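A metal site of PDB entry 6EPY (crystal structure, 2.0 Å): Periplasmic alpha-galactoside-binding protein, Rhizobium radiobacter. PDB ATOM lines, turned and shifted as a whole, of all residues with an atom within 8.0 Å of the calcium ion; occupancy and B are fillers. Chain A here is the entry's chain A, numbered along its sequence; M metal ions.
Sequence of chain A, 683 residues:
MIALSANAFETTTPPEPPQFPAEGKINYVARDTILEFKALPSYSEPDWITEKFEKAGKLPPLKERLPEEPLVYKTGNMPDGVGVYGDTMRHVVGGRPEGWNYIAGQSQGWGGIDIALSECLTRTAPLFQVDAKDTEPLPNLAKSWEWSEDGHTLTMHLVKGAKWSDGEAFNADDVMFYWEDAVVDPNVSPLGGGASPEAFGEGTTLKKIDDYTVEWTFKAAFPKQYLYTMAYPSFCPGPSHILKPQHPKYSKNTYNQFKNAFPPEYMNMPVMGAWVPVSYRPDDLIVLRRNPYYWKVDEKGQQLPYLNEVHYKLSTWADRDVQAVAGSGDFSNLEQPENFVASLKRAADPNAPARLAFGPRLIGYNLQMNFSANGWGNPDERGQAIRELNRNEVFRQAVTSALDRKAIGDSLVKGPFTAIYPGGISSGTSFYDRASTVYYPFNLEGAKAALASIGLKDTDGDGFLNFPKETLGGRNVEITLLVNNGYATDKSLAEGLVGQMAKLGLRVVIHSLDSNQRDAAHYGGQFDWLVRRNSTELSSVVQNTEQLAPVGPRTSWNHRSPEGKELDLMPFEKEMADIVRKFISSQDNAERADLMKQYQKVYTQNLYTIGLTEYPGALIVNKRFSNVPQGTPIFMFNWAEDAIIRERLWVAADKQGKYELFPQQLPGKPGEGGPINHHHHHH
Within 4 Å of the calcium ion: Asp 458, Asp 460, Asp 462, Phe 464, Asn 466 and Asn 476.
The side-chain carboxylate (OD1) of Asp 458 lies close to the backbone NH (N) of Gly 461, at 3.3 Å. OD1 of Asn 466 sits close to O of Gly 474. O of Lys 457 is in hydrogen-bond range of N of Asn 466, at 3.0 Å. The backbone NH (N) of Gly 463 is in hydrogen-bond range of the side-chain carboxylate (OD2) of Asp 458 (2.8 Å). The side-chain hydroxyl of Thr 459 sits close to the side-chain amide oxygen of Asn 466 (3.5 Å).
O of Phe 464 is bound to the calcium ion (2.2 Å). The side-chain carboxylate (OD1) of Asp 462 binds the calcium ion. The side-chain carboxylate (OD1) of Asp 460 binds the calcium ion (2.3 Å). The calcium ion is bound by OD1 of Asn 476 (2.3 Å). The side-chain carboxylate (OD1) of Asp 458 binds the calcium ion, 2.4 Å away. ND2 of Asn 466 binds the calcium ion (2.4 Å).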
ATOM      1  N   LYS A 457      -1.705 -17.123  -6.488  1.00  0.00           N
ATOM      2  CA  LYS A 457      -1.439 -15.775  -5.998  1.00  0.00           C
ATOM      3  C   LYS A 457      -2.030 -14.709  -6.953  1.00  0.00           C
ATOM      4  O   LYS A 457      -2.080 -14.934  -8.156  1.00  0.00           O
ATOM      5  CB  LYS A 457       0.100 -15.618  -5.809  1.00  0.00           C
ATOM      6  CG  LYS A 457       0.618 -14.247  -5.466  1.00  0.00           C
ATOM      7  CD  LYS A 457       2.102 -14.245  -5.683  1.00  0.00           C
ATOM      8  CE  LYS A 457       2.641 -12.860  -5.822  1.00  0.00           C
ATOM      9  NZ  LYS A 457       3.715 -12.819  -6.847  1.00  0.00           N
ATOM     10  N   ASP A 458      -2.464 -13.559  -6.397  1.00  0.00           N
ATOM     11  CA  ASP A 458      -3.018 -12.450  -7.165  1.00  0.00           C
ATOM     12  C   ASP A 458      -1.869 -11.692  -7.810  1.00  0.00           C
ATOM     13  O   ASP A 458      -1.080 -11.063  -7.107  1.00  0.00           O
ATOM     14  CB  ASP A 458      -3.888 -11.545  -6.262  1.00  0.00           C
ATOM     15  CG  ASP A 458      -4.517 -10.332  -6.929  1.00  0.00           C
ATOM     16  OD1 ASP A 458      -4.790 -10.390  -8.148  1.00  0.00           O
ATOM     17  OD2 ASP A 458      -4.809  -9.350  -6.218  1.00  0.00           O
ATOM     18  N   THR A 459      -1.724 -11.840  -9.133  1.00  0.00           N
ATOM     19  CA  THR A 459      -0.634 -11.235  -9.909  1.00  0.00           C
ATOM     20  C   THR A 459      -1.069  -9.965 -10.668  1.00  0.00           C
ATOM     21  O   THR A 459      -0.250  -9.380 -11.367  1.00  0.00           O
ATOM     22  CB  THR A 459       0.038 -12.287 -10.831  1.00  0.00           C
ATOM     23  OG1 THR A 459      -0.940 -12.840 -11.715  1.00  0.00           O
ATOM     24  CG2 THR A 459       0.734 -13.408 -10.048  1.00  0.00           C
ATOM     25  N   ASP A 460      -2.349  -9.542 -10.539  1.00  0.00           N
ATOM     26  CA  ASP A 460      -2.839  -8.354 -11.257  1.00  0.00           C
ATOM     27  C   ASP A 460      -3.527  -7.310 -10.319  1.00  0.00           C
ATOM     28  O   ASP A 460      -4.168  -6.368 -10.800  1.00  0.00           O
ATOM     29  CB  ASP A 460      -3.717  -8.760 -12.461  1.00  0.00           C
ATOM     30  CG  ASP A 460      -4.769  -9.817 -12.208  1.00  0.00           C
ATOM     31  OD1 ASP A 460      -5.425  -9.743 -11.162  1.00  0.00           O
ATOM     32  OD2 ASP A 460      -4.998 -10.675 -13.093  1.00  0.00           O
ATOM     33  N   GLY A 461      -3.379  -7.497  -9.011  1.00  0.00           N
ATOM     34  CA  GLY A 461      -3.925  -6.635  -7.970  1.00  0.00           C
ATOM     35  C   GLY A 461      -5.438  -6.486  -7.868  1.00  0.00           C
ATOM     36  O   GLY A 461      -5.927  -5.536  -7.234  1.00  0.00           O
ATOM     37  N   ASP A 462      -6.228  -7.413  -8.476  1.00  0.00           N
ATOM     38  CA  ASP A 462      -7.683  -7.291  -8.422  1.00  0.00           C
ATOM     39  C   ASP A 462      -8.318  -8.033  -7.220  1.00  0.00           C
ATOM     40  O   ASP A 462      -9.548  -8.111  -7.126  1.00  0.00           O
ATOM     41  CB  ASP A 462      -8.348  -7.680  -9.761  1.00  0.00           C
ATOM     42  CG  ASP A 462      -8.332  -9.153 -10.146  1.00  0.00           C
ATOM     43  OD1 ASP A 462      -7.678  -9.962  -9.436  1.00  0.00           O
ATOM     44  OD2 ASP A 462      -8.956  -9.504 -11.170  1.00  0.00           O
ATOM     45  N   GLY A 463      -7.483  -8.555  -6.323  1.00  0.00           N
ATOM     46  CA  GLY A 463      -7.932  -9.291  -5.139  1.00  0.00           C
ATOM     47  C   GLY A 463      -8.329 -10.746  -5.379  1.00  0.00           C
ATOM     48  O   GLY A 463      -8.668 -11.436  -4.426  1.00  0.00           O
ATOM     49  N   PHE A 464      -8.283 -11.194  -6.642  1.00  0.00           N
ATOM     50  CA  PHE A 464      -8.596 -12.558  -7.027  1.00  0.00           C
ATOM     51  C   PHE A 464      -7.342 -13.315  -7.413  1.00  0.00           C
ATOM     52  O   PHE A 464      -6.493 -12.794  -8.123  1.00  0.00           O
ATOM     53  CB  PHE A 464      -9.656 -12.623  -8.132  1.00  0.00           C
ATOM     54  CG  PHE A 464     -11.029 -12.229  -7.656  1.00  0.00           C
ATOM     55  CD1 PHE A 464     -11.782 -13.098  -6.876  1.00  0.00           C
ATOM     56  CD2 PHE A 464     -11.567 -10.992  -7.966  1.00  0.00           C
ATOM     57  CE1 PHE A 464     -13.055 -12.728  -6.430  1.00  0.00           C
ATOM     58  CE2 PHE A 464     -12.836 -10.635  -7.523  1.00  0.00           C
ATOM     59  CZ  PHE A 464     -13.579 -11.512  -6.774  1.00  0.00           C
ATOM     60  N   LEU A 465      -7.212 -14.533  -6.908  1.00  0.00           N
ATOM     61  CA  LEU A 465      -6.054 -15.383  -7.177  1.00  0.00           C
ATOM     62  C   LEU A 465      -5.961 -15.809  -8.638  1.00  0.00           C
ATOM     63  O   LEU A 465      -6.967 -16.105  -9.303  1.00  0.00           O
ATOM     64  CB  LEU A 465      -6.028 -16.597  -6.226  1.00  0.00           C
ATOM     65  CG  LEU A 465      -6.010 -16.272  -4.712  1.00  0.00           C
ATOM     66  CD1 LEU A 465      -6.126 -17.545  -3.900  1.00  0.00           C
ATOM     67  CD2 LEU A 465      -4.770 -15.500  -4.306  1.00  0.00           C
ATOM     68  N   ASN A 466      -4.733 -15.788  -9.141  1.00  0.00           N
ATOM     69  CA  ASN A 466      -4.398 -16.180 -10.495  1.00  0.00           C
ATOM     70  C   ASN A 466      -3.762 -17.552 -10.471  1.00  0.00           C
ATOM     71  O   ASN A 466      -3.073 -17.890  -9.505  1.00  0.00           O
ATOM     72  CB  ASN A 466      -3.401 -15.191 -11.093  1.00  0.00           C
ATOM     73  CG  ASN A 466      -3.985 -13.846 -11.414  1.00  0.00           C
ATOM     74  OD1 ASN A 466      -4.249 -13.545 -12.572  1.00  0.00           O
ATOM     75  ND2 ASN A 466      -4.249 -13.021 -10.408  1.00  0.00           N
ATOM     76  N   PHE A 467      -3.937 -18.310 -11.560  1.00  0.00           N
ATOM     77  CA  PHE A 467      -3.238 -19.580 -11.742  1.00  0.00           C
ATOM     78  C   PHE A 467      -1.759 -19.229 -11.954  1.00  0.00           C
ATOM     79  O   PHE A 467      -1.481 -18.120 -12.412  1.00  0.00           O
ATOM     80  CB  PHE A 467      -3.714 -20.259 -13.054  1.00  0.00           C
ATOM     81  CG  PHE A 467      -5.032 -20.971 -12.991  1.00  0.00           C
ATOM     82  CD1 PHE A 467      -5.149 -22.190 -12.330  1.00  0.00           C
ATOM     83  CD2 PHE A 467      -6.152 -20.462 -13.628  1.00  0.00           C
ATOM     84  CE1 PHE A 467      -6.373 -22.870 -12.290  1.00  0.00           C
ATOM     85  CE2 PHE A 467      -7.372 -21.120 -13.579  1.00  0.00           C
ATOM     86  CZ  PHE A 467      -7.469 -22.339 -12.928  1.00  0.00           C
ATOM     87  N   GLY A 474      -1.765 -17.819 -16.799  1.00  0.00           N
ATOM     88  CA  GLY A 474      -1.742 -17.146 -15.505  1.00  0.00           C
ATOM     89  C   GLY A 474      -2.951 -16.262 -15.219  1.00  0.00           C
ATOM     90  O   GLY A 474      -2.839 -15.324 -14.409  1.00  0.00           O
ATOM     91  N   ARG A 475      -4.116 -16.544 -15.853  1.00  0.00           N
ATOM     92  CA  ARG A 475      -5.359 -15.778 -15.647  1.00  0.00           C
ATOM     93  C   ARG A 475      -5.961 -16.068 -14.262  1.00  0.00           C
ATOM     94  O   ARG A 475      -5.561 -17.015 -13.583  1.00  0.00           O
ATOM     95  CB  ARG A 475      -6.387 -16.085 -16.769  1.00  0.00           C
ATOM     96  CG  ARG A 475      -7.096 -17.421 -16.601  1.00  0.00           C
ATOM     97  CD  ARG A 475      -8.104 -17.712 -17.696  1.00  0.00           C
ATOM     98  NE  ARG A 475      -7.401 -18.096 -18.920  1.00  0.00           N
ATOM     99  CZ  ARG A 475      -7.921 -18.852 -19.868  1.00  0.00           C
ATOM    100  NH1 ARG A 475      -9.158 -19.306 -19.772  1.00  0.00           N
ATOM    101  NH2 ARG A 475      -7.192 -19.163 -20.929  1.00  0.00           N
ATOM    102  N   ASN A 476      -6.964 -15.267 -13.862  1.00  0.00           N
ATOM    103  CA  ASN A 476      -7.684 -15.484 -12.596  1.00  0.00           C
ATOM    104  C   ASN A 476      -8.371 -16.842 -12.584  1.00  0.00           C
ATOM    105  O   ASN A 476      -8.939 -17.267 -13.596  1.00  0.00           O
ATOM    106  CB  ASN A 476      -8.753 -14.409 -12.407  1.00  0.00           C
ATOM    107  CG  ASN A 476      -8.253 -13.114 -11.848  1.00  0.00           C
ATOM    108  OD1 ASN A 476      -7.236 -13.042 -11.152  1.00  0.00           O
ATOM    109  ND2 ASN A 476      -9.006 -12.067 -12.071  1.00  0.00           N
ATOM    110  N   VAL A 477      -8.337 -17.511 -11.422  1.00  0.00           N
ATOM    111  CA  VAL A 477      -9.057 -18.767 -11.215  1.00  0.00           C
ATOM    112  C   VAL A 477     -10.559 -18.398 -11.263  1.00  0.00           C
ATOM    113  O   VAL A 477     -10.976 -17.411 -10.634  1.00  0.00           O
ATOM    114  CB  VAL A 477      -8.668 -19.434  -9.857  1.00  0.00           C
ATOM    115  CG1 VAL A 477      -9.501 -20.676  -9.575  1.00  0.00           C
ATOM    116  CG2 VAL A 477      -7.172 -19.753  -9.810  1.00  0.00           C
ATOM    117  N   GLY A 505     -10.163 -15.092  -1.973  1.00  0.00           N
ATOM    118  CA  GLY A 505      -9.555 -14.721  -3.242  1.00  0.00           C
ATOM    119  C   GLY A 505      -9.948 -15.589  -4.428  1.00  0.00           C
ATOM    120  O   GLY A 505      -9.358 -15.493  -5.496  1.00  0.00           O
HETATM  121 CA    CA M   1      -6.062 -11.509  -9.853  1.00  0.00          CA
